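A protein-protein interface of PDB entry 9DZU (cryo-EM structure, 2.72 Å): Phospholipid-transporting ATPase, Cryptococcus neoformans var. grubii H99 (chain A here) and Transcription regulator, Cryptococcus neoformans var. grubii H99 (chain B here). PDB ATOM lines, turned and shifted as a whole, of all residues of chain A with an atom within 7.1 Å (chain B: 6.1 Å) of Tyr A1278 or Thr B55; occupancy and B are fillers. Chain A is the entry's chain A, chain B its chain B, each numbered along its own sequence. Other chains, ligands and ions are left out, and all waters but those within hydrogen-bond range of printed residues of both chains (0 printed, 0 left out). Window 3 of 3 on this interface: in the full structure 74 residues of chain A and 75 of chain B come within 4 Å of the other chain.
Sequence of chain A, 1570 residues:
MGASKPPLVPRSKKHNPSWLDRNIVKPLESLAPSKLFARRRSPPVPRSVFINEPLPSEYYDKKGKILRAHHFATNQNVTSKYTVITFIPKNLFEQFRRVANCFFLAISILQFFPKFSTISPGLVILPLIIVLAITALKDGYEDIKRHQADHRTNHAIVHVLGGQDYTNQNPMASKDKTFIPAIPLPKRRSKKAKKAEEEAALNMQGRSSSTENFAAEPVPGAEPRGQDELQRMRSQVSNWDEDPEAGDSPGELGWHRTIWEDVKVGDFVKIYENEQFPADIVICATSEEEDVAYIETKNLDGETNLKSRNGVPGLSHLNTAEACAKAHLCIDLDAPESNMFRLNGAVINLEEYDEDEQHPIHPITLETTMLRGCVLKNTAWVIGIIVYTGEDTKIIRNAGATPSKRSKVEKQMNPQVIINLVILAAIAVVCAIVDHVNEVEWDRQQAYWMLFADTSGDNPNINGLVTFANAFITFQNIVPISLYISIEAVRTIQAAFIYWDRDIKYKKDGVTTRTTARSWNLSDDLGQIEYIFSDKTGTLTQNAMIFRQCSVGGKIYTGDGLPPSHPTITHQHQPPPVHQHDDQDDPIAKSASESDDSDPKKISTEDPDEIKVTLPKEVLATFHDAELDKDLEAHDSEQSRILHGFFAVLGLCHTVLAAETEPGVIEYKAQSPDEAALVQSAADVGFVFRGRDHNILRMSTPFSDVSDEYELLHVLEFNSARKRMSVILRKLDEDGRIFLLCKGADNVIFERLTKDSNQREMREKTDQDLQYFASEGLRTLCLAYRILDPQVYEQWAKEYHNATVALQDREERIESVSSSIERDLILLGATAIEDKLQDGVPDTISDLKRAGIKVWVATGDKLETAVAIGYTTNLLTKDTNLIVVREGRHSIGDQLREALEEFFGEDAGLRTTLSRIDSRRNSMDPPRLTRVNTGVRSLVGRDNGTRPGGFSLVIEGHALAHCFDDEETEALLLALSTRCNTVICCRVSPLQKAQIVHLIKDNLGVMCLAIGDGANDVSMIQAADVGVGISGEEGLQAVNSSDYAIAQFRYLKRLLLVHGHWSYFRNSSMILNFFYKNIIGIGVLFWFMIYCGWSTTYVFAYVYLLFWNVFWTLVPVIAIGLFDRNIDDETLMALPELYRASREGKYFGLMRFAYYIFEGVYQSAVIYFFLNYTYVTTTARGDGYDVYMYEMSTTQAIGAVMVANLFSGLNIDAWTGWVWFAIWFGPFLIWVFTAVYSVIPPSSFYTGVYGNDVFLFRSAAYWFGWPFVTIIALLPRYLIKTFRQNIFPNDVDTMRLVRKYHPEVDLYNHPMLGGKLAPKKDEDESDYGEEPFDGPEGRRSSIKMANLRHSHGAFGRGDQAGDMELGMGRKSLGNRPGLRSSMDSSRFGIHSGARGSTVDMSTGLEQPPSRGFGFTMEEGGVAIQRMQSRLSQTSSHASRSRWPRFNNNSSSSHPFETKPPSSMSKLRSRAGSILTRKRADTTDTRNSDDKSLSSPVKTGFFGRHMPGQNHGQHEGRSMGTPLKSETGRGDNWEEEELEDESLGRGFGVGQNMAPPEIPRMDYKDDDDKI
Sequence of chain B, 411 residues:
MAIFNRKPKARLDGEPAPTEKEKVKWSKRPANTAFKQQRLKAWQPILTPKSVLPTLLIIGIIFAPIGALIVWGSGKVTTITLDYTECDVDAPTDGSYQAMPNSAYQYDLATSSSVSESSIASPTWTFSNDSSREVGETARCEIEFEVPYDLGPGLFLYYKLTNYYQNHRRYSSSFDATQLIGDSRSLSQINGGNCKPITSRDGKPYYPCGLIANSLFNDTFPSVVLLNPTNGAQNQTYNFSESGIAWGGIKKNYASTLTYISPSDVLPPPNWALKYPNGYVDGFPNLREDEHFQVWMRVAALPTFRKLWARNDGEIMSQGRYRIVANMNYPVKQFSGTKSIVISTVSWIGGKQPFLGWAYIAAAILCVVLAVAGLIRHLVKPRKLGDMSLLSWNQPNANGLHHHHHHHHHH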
ATOM      1  N   TYR A1155     -20.979   5.948 -37.687  1.00  0.00           N
ATOM      2  CA  TYR A1155     -20.291   6.455 -36.506  1.00  0.00           C
ATOM      3  C   TYR A1155     -21.274   7.102 -35.541  1.00  0.00           C
ATOM      4  O   TYR A1155     -21.225   6.858 -34.332  1.00  0.00           O
ATOM      5  CB  TYR A1155     -19.205   7.449 -36.909  1.00  0.00           C
ATOM      6  CG  TYR A1155     -18.639   8.233 -35.745  1.00  0.00           C
ATOM      7  CD1 TYR A1155     -17.725   7.659 -34.876  1.00  0.00           C
ATOM      8  CD2 TYR A1155     -19.017   9.547 -35.519  1.00  0.00           C
ATOM      9  CE1 TYR A1155     -17.207   8.369 -33.814  1.00  0.00           C
ATOM     10  CE2 TYR A1155     -18.504  10.265 -34.459  1.00  0.00           C
ATOM     11  CZ  TYR A1155     -17.599   9.670 -33.609  1.00  0.00           C
ATOM     12  OH  TYR A1155     -17.084  10.381 -32.551  1.00  0.00           O
ATOM     13  N   GLU A1159     -22.208   5.709 -31.872  1.00  0.00           N
ATOM     14  CA  GLU A1159     -22.031   6.597 -30.728  1.00  0.00           C
ATOM     15  C   GLU A1159     -23.305   6.679 -29.901  1.00  0.00           C
ATOM     16  O   GLU A1159     -23.260   6.602 -28.668  1.00  0.00           O
ATOM     17  CB  GLU A1159     -21.617   7.992 -31.200  1.00  0.00           C
ATOM     18  CG  GLU A1159     -20.150   8.127 -31.568  1.00  0.00           C
ATOM     19  CD  GLU A1159     -19.258   8.293 -30.355  1.00  0.00           C
ATOM     20  OE1 GLU A1159     -19.790   8.547 -29.254  1.00  0.00           O
ATOM     21  OE2 GLU A1159     -18.023   8.170 -30.502  1.00  0.00           O
ATOM     22  N   PHE A1207     -23.662  16.626 -26.616  1.00  0.00           N
ATOM     23  CA  PHE A1207     -23.039  16.071 -27.812  1.00  0.00           C
ATOM     24  C   PHE A1207     -23.232  16.999 -29.001  1.00  0.00           C
ATOM     25  O   PHE A1207     -22.277  17.294 -29.738  1.00  0.00           O
ATOM     26  CB  PHE A1207     -23.632  14.693 -28.099  1.00  0.00           C
ATOM     27  CG  PHE A1207     -22.984  13.966 -29.237  1.00  0.00           C
ATOM     28  CD1 PHE A1207     -21.917  13.120 -29.014  1.00  0.00           C
ATOM     29  CD2 PHE A1207     -23.461  14.101 -30.528  1.00  0.00           C
ATOM     30  CE1 PHE A1207     -21.330  12.439 -30.054  1.00  0.00           C
ATOM     31  CE2 PHE A1207     -22.874  13.422 -31.571  1.00  0.00           C
ATOM     32  CZ  PHE A1207     -21.808  12.592 -31.333  1.00  0.00           C
ATOM     33  N   LEU A1210     -20.924  19.927 -28.559  1.00  0.00           N
ATOM     34  CA  LEU A1210     -19.552  19.593 -28.926  1.00  0.00           C
ATOM     35  C   LEU A1210     -19.389  19.523 -30.436  1.00  0.00           C
ATOM     36  O   LEU A1210     -18.306  19.794 -30.965  1.00  0.00           O
ATOM     37  CB  LEU A1210     -19.136  18.267 -28.290  1.00  0.00           C
ATOM     38  CG  LEU A1210     -18.628  18.287 -26.851  1.00  0.00           C
ATOM     39  CD1 LEU A1210     -18.254  16.885 -26.414  1.00  0.00           C
ATOM     40  CD2 LEU A1210     -17.442  19.224 -26.713  1.00  0.00           C
ATOM     41  N   ALA A1273     -20.498   9.203 -21.053  1.00  0.00           N
ATOM     42  CA  ALA A1273     -21.013   9.129 -22.413  1.00  0.00           C
ATOM     43  C   ALA A1273     -20.269  10.078 -23.341  1.00  0.00           C
ATOM     44  O   ALA A1273     -20.010   9.739 -24.501  1.00  0.00           O
ATOM     45  CB  ALA A1273     -22.510   9.430 -22.421  1.00  0.00           C
ATOM     46  N   LEU A1274     -19.912  11.268 -22.857  1.00  0.00           N
ATOM     47  CA  LEU A1274     -19.319  12.267 -23.733  1.00  0.00           C
ATOM     48  C   LEU A1274     -17.796  12.241 -23.763  1.00  0.00           C
ATOM     49  O   LEU A1274     -17.204  12.941 -24.591  1.00  0.00           O
ATOM     50  CB  LEU A1274     -19.786  13.661 -23.319  1.00  0.00           C
ATOM     51  CG  LEU A1274     -21.294  13.865 -23.388  1.00  0.00           C
ATOM     52  CD1 LEU A1274     -21.648  15.147 -22.693  1.00  0.00           C
ATOM     53  CD2 LEU A1274     -21.763  13.887 -24.827  1.00  0.00           C
ATOM     54  N   LEU A1275     -17.151  11.472 -22.890  1.00  0.00           N
ATOM     55  CA  LEU A1275     -15.690  11.436 -22.893  1.00  0.00           C
ATOM     56  C   LEU A1275     -15.108  10.886 -24.190  1.00  0.00           C
ATOM     57  O   LEU A1275     -14.172  11.507 -24.729  1.00  0.00           O
ATOM     58  CB  LEU A1275     -15.197  10.648 -21.675  1.00  0.00           C
ATOM     59  CG  LEU A1275     -13.718  10.805 -21.340  1.00  0.00           C
ATOM     60  CD1 LEU A1275     -13.422  12.247 -20.982  1.00  0.00           C
ATOM     61  CD2 LEU A1275     -13.324   9.875 -20.212  1.00  0.00           C
ATOM     62  N   PRO A1276     -15.571   9.750 -24.733  1.00  0.00           N
ATOM     63  CA  PRO A1276     -15.002   9.287 -26.008  1.00  0.00           C
ATOM     64  C   PRO A1276     -15.144  10.290 -27.136  1.00  0.00           C
ATOM     65  O   PRO A1276     -14.214  10.444 -27.931  1.00  0.00           O
ATOM     66  CB  PRO A1276     -15.788   8.002 -26.290  1.00  0.00           C
ATOM     67  CG  PRO A1276     -16.222   7.535 -24.964  1.00  0.00           C
ATOM     68  CD  PRO A1276     -16.535   8.774 -24.197  1.00  0.00           C
ATOM     69  N   ARG A1277     -16.279  10.986 -27.223  1.00  0.00           N
ATOM     70  CA  ARG A1277     -16.454  11.976 -28.282  1.00  0.00           C
ATOM     71  C   ARG A1277     -15.479  13.133 -28.122  1.00  0.00           C
ATOM     72  O   ARG A1277     -14.879  13.589 -29.102  1.00  0.00           O
ATOM     73  CB  ARG A1277     -17.892  12.488 -28.290  1.00  0.00           C
ATOM     74  CG  ARG A1277     -18.150  13.583 -29.307  1.00  0.00           C
ATOM     75  CD  ARG A1277     -17.791  13.124 -30.706  1.00  0.00           C
ATOM     76  NE  ARG A1277     -18.112  14.129 -31.710  1.00  0.00           N
ATOM     77  CZ  ARG A1277     -17.765  14.047 -32.986  1.00  0.00           C
ATOM     78  NH1 ARG A1277     -17.071  13.022 -33.449  1.00  0.00           N
ATOM     79  NH2 ARG A1277     -18.120  15.022 -33.819  1.00  0.00           N
ATOM     80  N   TYR A1278     -15.306  13.615 -26.892  1.00  0.00           N
ATOM     81  CA  TYR A1278     -14.373  14.704 -26.632  1.00  0.00           C
ATOM     82  C   TYR A1278     -12.952  14.307 -27.014  1.00  0.00           C
ATOM     83  O   TYR A1278     -12.251  15.046 -27.721  1.00  0.00           O
ATOM     84  CB  TYR A1278     -14.465  15.096 -25.157  1.00  0.00           C
ATOM     85  CG  TYR A1278     -13.671  16.308 -24.741  1.00  0.00           C
ATOM     86  CD1 TYR A1278     -13.922  17.553 -25.297  1.00  0.00           C
ATOM     87  CD2 TYR A1278     -12.696  16.212 -23.762  1.00  0.00           C
ATOM     88  CE1 TYR A1278     -13.203  18.664 -24.905  1.00  0.00           C
ATOM     89  CE2 TYR A1278     -11.974  17.314 -23.364  1.00  0.00           C
ATOM     90  CZ  TYR A1278     -12.231  18.538 -23.937  1.00  0.00           C
ATOM     91  OH  TYR A1278     -11.509  19.641 -23.540  1.00  0.00           O
ATOM     92  N   LEU A1279     -12.521  13.121 -26.579  1.00  0.00           N
ATOM     93  CA  LEU A1279     -11.167  12.671 -26.886  1.00  0.00           C
ATOM     94  C   LEU A1279     -10.981  12.441 -28.380  1.00  0.00           C
ATOM     95  O   LEU A1279      -9.941  12.798 -28.945  1.00  0.00           O
ATOM     96  CB  LEU A1279     -10.846  11.405 -26.097  1.00  0.00           C
ATOM     97  CG  LEU A1279     -10.763  11.574 -24.580  1.00  0.00           C
ATOM     98  CD1 LEU A1279     -10.417  10.257 -23.919  1.00  0.00           C
ATOM     99  CD2 LEU A1279      -9.749  12.635 -24.214  1.00  0.00           C
ATOM    100  N   ILE A1280     -11.980  11.846 -29.039  1.00  0.00           N
ATOM    101  CA  ILE A1280     -11.891  11.598 -30.474  1.00  0.00           C
ATOM    102  C   ILE A1280     -11.785  12.909 -31.234  1.00  0.00           C
ATOM    103  O   ILE A1280     -10.964  13.044 -32.147  1.00  0.00           O
ATOM    104  CB  ILE A1280     -13.097  10.766 -30.949  1.00  0.00           C
ATOM    105  CG1 ILE A1280     -12.910   9.294 -30.587  1.00  0.00           C
ATOM    106  CG2 ILE A1280     -13.305  10.924 -32.441  1.00  0.00           C
ATOM    107  CD1 ILE A1280     -14.060   8.415 -31.016  1.00  0.00           C
ATOM    108  N   LYS A1281     -12.605  13.895 -30.873  1.00  0.00           N
ATOM    109  CA  LYS A1281     -12.564  15.179 -31.561  1.00  0.00           C
ATOM    110  C   LYS A1281     -11.214  15.857 -31.368  1.00  0.00           C
ATOM    111  O   LYS A1281     -10.608  16.345 -32.332  1.00  0.00           O
ATOM    112  CB  LYS A1281     -13.700  16.070 -31.062  1.00  0.00           C
ATOM    113  CG  LYS A1281     -13.981  17.261 -31.945  1.00  0.00           C
ATOM    114  CD  LYS A1281     -15.279  17.933 -31.558  1.00  0.00           C
ATOM    115  CE  LYS A1281     -15.625  19.041 -32.538  1.00  0.00           C
ATOM    116  NZ  LYS A1281     -14.557  20.075 -32.604  1.00  0.00           N
ATOM    117  N   THR A1282     -10.711  15.872 -30.131  1.00  0.00           N
ATOM    118  CA  THR A1282      -9.424  16.508 -29.869  1.00  0.00           C
ATOM    119  C   THR A1282      -8.300  15.829 -30.645  1.00  0.00           C
ATOM    120  O   THR A1282      -7.490  16.496 -31.301  1.00  0.00           O
ATOM    121  CB  THR A1282      -9.127  16.494 -28.370  1.00  0.00           C
ATOM    122  OG1 THR A1282     -10.054  17.347 -27.692  1.00  0.00           O
ATOM    123  CG2 THR A1282      -7.710  16.977 -28.104  1.00  0.00           C
ATOM    124  N   PHE A1283      -8.244  14.498 -30.598  1.00  0.00           N
ATOM    125  CA  PHE A1283      -7.151  13.791 -31.255  1.00  0.00           C
ATOM    126  C   PHE A1283      -7.267  13.844 -32.771  1.00  0.00           C
ATOM    127  O   PHE A1283      -6.246  13.871 -33.463  1.00  0.00           O
ATOM    128  CB  PHE A1283      -7.092  12.346 -30.769  1.00  0.00           C
ATOM    129  CG  PHE A1283      -6.632  12.209 -29.347  1.00  0.00           C
ATOM    130  CD1 PHE A1283      -5.972  13.252 -28.716  1.00  0.00           C
ATOM    131  CD2 PHE A1283      -6.857  11.039 -28.641  1.00  0.00           C
ATOM    132  CE1 PHE A1283      -5.549  13.132 -27.411  1.00  0.00           C
ATOM    133  CE2 PHE A1283      -6.435  10.913 -27.332  1.00  0.00           C
ATOM    134  CZ  PHE A1283      -5.779  11.962 -26.716  1.00  0.00           C
ATOM    135  N   ARG A1284      -8.486  13.860 -33.310  1.00  0.00           N
ATOM    136  CA  ARG A1284      -8.647  14.018 -34.749  1.00  0.00           C
ATOM    137  C   ARG A1284      -8.203  15.403 -35.197  1.00  0.00           C
ATOM    138  O   ARG A1284      -7.566  15.545 -36.246  1.00  0.00           O
ATOM    139  CB  ARG A1284     -10.100  13.765 -35.147  1.00  0.00           C
ATOM    140  CG  ARG A1284     -10.302  13.545 -36.632  1.00  0.00           C
ATOM    141  CD  ARG A1284     -11.769  13.626 -37.012  1.00  0.00           C
ATOM    142  NE  ARG A1284     -12.288  14.982 -36.881  1.00  0.00           N
ATOM    143  CZ  ARG A1284     -12.189  15.915 -37.820  1.00  0.00           C
ATOM    144  NH1 ARG A1284     -11.592  15.671 -38.975  1.00  0.00           N
ATOM    145  NH2 ARG A1284     -12.702  17.120 -37.593  1.00  0.00           N
ATOM    146  N   THR B  48      -5.021  22.508 -28.280  1.00  0.00           N
ATOM    147  CA  THR B  48      -6.265  21.947 -27.761  1.00  0.00           C
ATOM    148  C   THR B  48      -6.045  20.915 -26.638  1.00  0.00           C
ATOM    149  O   THR B  48      -6.741  20.977 -25.624  1.00  0.00           O
ATOM    150  CB  THR B  48      -7.106  21.308 -28.890  1.00  0.00           C
ATOM    151  OG1 THR B  48      -7.314  22.267 -29.935  1.00  0.00           O
ATOM    152  CG2 THR B  48      -8.455  20.848 -28.360  1.00  0.00           C
ATOM    153  N   SER B  51      -5.896  22.125 -23.232  1.00  0.00           N
ATOM    154  CA  SER B  51      -7.170  22.298 -22.549  1.00  0.00           C
ATOM    155  C   SER B  51      -7.926  20.988 -22.376  1.00  0.00           C
ATOM    156  O   SER B  51      -9.094  21.012 -21.977  1.00  0.00           O
ATOM    157  CB  SER B  51      -8.045  23.303 -23.306  1.00  0.00           C
ATOM    158  OG  SER B  51      -8.299  22.864 -24.630  1.00  0.00           O
ATOM    159  N   VAL B  52      -7.297  19.854 -22.666  1.00  0.00           N
ATOM    160  CA  VAL B  52      -7.935  18.548 -22.558  1.00  0.00           C
ATOM    161  C   VAL B  52      -7.347  17.731 -21.417  1.00  0.00           C
ATOM    162  O   VAL B  52      -8.080  17.130 -20.632  1.00  0.00           O
ATOM    163  CB  VAL B  52      -7.827  17.793 -23.902  1.00  0.00           C
ATOM    164  CG1 VAL B  52      -8.176  16.323 -23.725  1.00  0.00           C
ATOM    165  CG2 VAL B  52      -8.729  18.441 -24.936  1.00  0.00           C
ATOM    166  N   LEU B  53      -6.020  17.694 -21.316  1.00  0.00           N
ATOM    167  CA  LEU B  53      -5.381  16.974 -20.216  1.00  0.00           C
ATOM    168  C   LEU B  53      -5.768  17.521 -18.846  1.00  0.00           C
ATOM    169  O   LEU B  53      -6.100  16.716 -17.955  1.00  0.00           O
ATOM    170  CB  LEU B  53      -3.862  16.974 -20.417  1.00  0.00           C
ATOM    171  CG  LEU B  53      -3.230  15.880 -21.285  1.00  0.00           C
ATOM    172  CD1 LEU B  53      -3.915  15.742 -22.637  1.00  0.00           C
ATOM    173  CD2 LEU B  53      -1.755  16.174 -21.472  1.00  0.00           C
ATOM    174  N   PRO B  54      -5.746  18.837 -18.595  1.00  0.00           N
ATOM    175  CA  PRO B  54      -6.245  19.323 -17.301  1.00  0.00           C
ATOM    176  C   PRO B  54      -7.699  18.978 -17.058  1.00  0.00           C
ATOM    177  O   PRO B  54      -8.089  18.776 -15.905  1.00  0.00           O
ATOM    178  CB  PRO B  54      -6.029  20.839 -17.385  1.00  0.00           C
ATOM    179  CG  PRO B  54      -5.961  21.131 -18.831  1.00  0.00           C
ATOM    180  CD  PRO B  54      -5.265  19.952 -19.428  1.00  0.00           C
ATOM    181  N   THR B  55      -8.516  18.901 -18.109  1.00  0.00           N
ATOM    182  CA  THR B  55      -9.902  18.479 -17.931  1.00  0.00           C
ATOM    183  C   THR B  55      -9.977  17.049 -17.410  1.00  0.00           C
ATOM    184  O   THR B  55     -10.752  16.759 -16.492  1.00  0.00           O
ATOM    185  CB  THR B  55     -10.668  18.615 -19.245  1.00  0.00           C
ATOM    186  OG1 THR B  55     -10.683  19.990 -19.649  1.00  0.00           O
ATOM    187  CG2 THR B  55     -12.099  18.128 -19.080  1.00  0.00           C
ATOM    188  N   LEU B  56      -9.171  16.145 -17.971  1.00  0.00           N
ATOM    189  CA  LEU B  56      -9.137  14.774 -17.471  1.00  0.00           C
ATOM    190  C   LEU B  56      -8.648  14.722 -16.030  1.00  0.00           C
ATOM    191  O   LEU B  56      -9.205  13.984 -15.205  1.00  0.00           O
ATOM    192  CB  LEU B  56      -8.250  13.906 -18.361  1.00  0.00           C
ATOM    193  CG  LEU B  56      -8.767  13.554 -19.754  1.00  0.00           C
ATOM    194  CD1 LEU B  56      -7.757  12.695 -20.488  1.00  0.00           C
ATOM    195  CD2 LEU B  56     -10.095  12.838 -19.651  1.00  0.00           C
ATOM    196  N   LEU B  57      -7.607  15.494 -15.707  1.00  0.00           N
ATOM    197  CA  LEU B  57      -7.106  15.506 -14.335  1.00  0.00           C
ATOM    198  C   LEU B  57      -8.166  16.008 -13.363  1.00  0.00           C
ATOM    199  O   LEU B  57      -8.352  15.431 -12.286  1.00  0.00           O
ATOM    200  CB  LEU B  57      -5.844  16.358 -14.239  1.00  0.00           C
ATOM    201  CG  LEU B  57      -4.573  15.737 -14.813  1.00  0.00           C
ATOM    202  CD1 LEU B  57      -3.409  16.711 -14.724  1.00  0.00           C
ATOM    203  CD2 LEU B  57      -4.252  14.448 -14.084  1.00  0.00           C
ATOM    204  N   ILE B  58      -8.872  17.080 -13.726  1.00  0.00           N
ATOM    205  CA  ILE B  58      -9.915  17.623 -12.860  1.00  0.00           C
ATOM    206  C   ILE B  58     -11.052  16.624 -12.704  1.00  0.00           C
ATOM    207  O   ILE B  58     -11.587  16.437 -11.605  1.00  0.00           O
ATOM    208  CB  ILE B  58     -10.413  18.974 -13.407  1.00  0.00           C
ATOM    209  CG1 ILE B  58      -9.323  20.036 -13.268  1.00  0.00           C
ATOM    210  CG2 ILE B  58     -11.675  19.414 -12.690  1.00  0.00           C
ATOM    211  CD1 ILE B  58      -9.714  21.388 -13.822  1.00  0.00           C
ATOM    212  N   ILE B  59     -11.433  15.958 -13.797  1.00  0.00           N
ATOM    213  CA  ILE B  59     -12.500  14.964 -13.728  1.00  0.00           C
ATOM    214  C   ILE B  59     -12.116  13.844 -12.773  1.00  0.00           C
ATOM    215  O   ILE B  59     -12.919  13.419 -11.938  1.00  0.00           O
ATOM    216  CB  ILE B  59     -12.831  14.427 -15.132  1.00  0.00           C
ATOM    217  CG1 ILE B  59     -13.629  15.462 -15.926  1.00  0.00           C
ATOM    218  CG2 ILE B  59     -13.604  13.125 -15.041  1.00  0.00           C
ATOM    219  CD1 ILE B  59     -13.990  15.010 -17.323  1.00  0.00           C
ATOM    220  N   GLY B  60     -10.878  13.359 -12.869  1.00  0.00           N
ATOM    221  CA  GLY B  60     -10.449  12.295 -11.973  1.00  0.00           C
ATOM    222  C   GLY B  60     -10.382  12.736 -10.521  1.00  0.00           C
ATOM    223  O   GLY B  60     -10.853  12.034  -9.619  1.00  0.00           O
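OH of Tyr A1278 lies within hydrogen-bond range of O of Ser B51 (3.2 Å).
The side-chain hydroxyl of Thr A1282 is in hydrogen-bond range of the backbone carbonyl oxygen of Tyr A1278, 3.2 Å away. The backbone carbonyl oxygen of Ser B51 is in hydrogen-bond range of the side-chain hydroxyl of Thr B55 (3.0 Å). O of Thr B48 sits at hydrogen-bond distance from OG of Ser B51.
Among the printed residues, merely in contact across the chains: Thr A1282 with Val B52, Tyr A1278 with Val B52, Leu A1275 with Leu B56, Thr A1282 with Thr B48 and Tyr A1278 with Thr B55.
Of the printed residues of chain B, Tyr A1278 touches Ser B51 (3.2 Å), Val B52 (3.3 Å) and Thr B55 (3.99 Å). Printed residues of chain A within 4 Å of Thr B55: Tyr A1278 (3.99 Å). Printed residues of chain B within 4 Å of Thr A1282: Thr B48 and Val B52. Of the printed residues of chain B, Leu A1275 touches Leu B56. Of the printed residues of chain A, Val B52 touches Tyr A1278 (3.3 Å) and Thr A1282 (3.2 Å). Printed residues of chain A within 4 Å of Ser B51: Tyr A1278 (3.2 Å). Leu B53 touches none of the printed residues of chain A. Ile B58 touches none of the printed residues of chain A.
Of the 11 printed residues of chain B, 5 touch a printed residue of chain A. Along chain B the printed residues that touch a printed residue of chain A span positions 48 to 56. Along chain A the printed residues that touch a printed residue of chain B span positions 1275 to 1282. Among the printed residues, no Asp or Glu carboxylate lies within 4 Å of a Lys or Arg side-chain nitrogen of the other chain.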
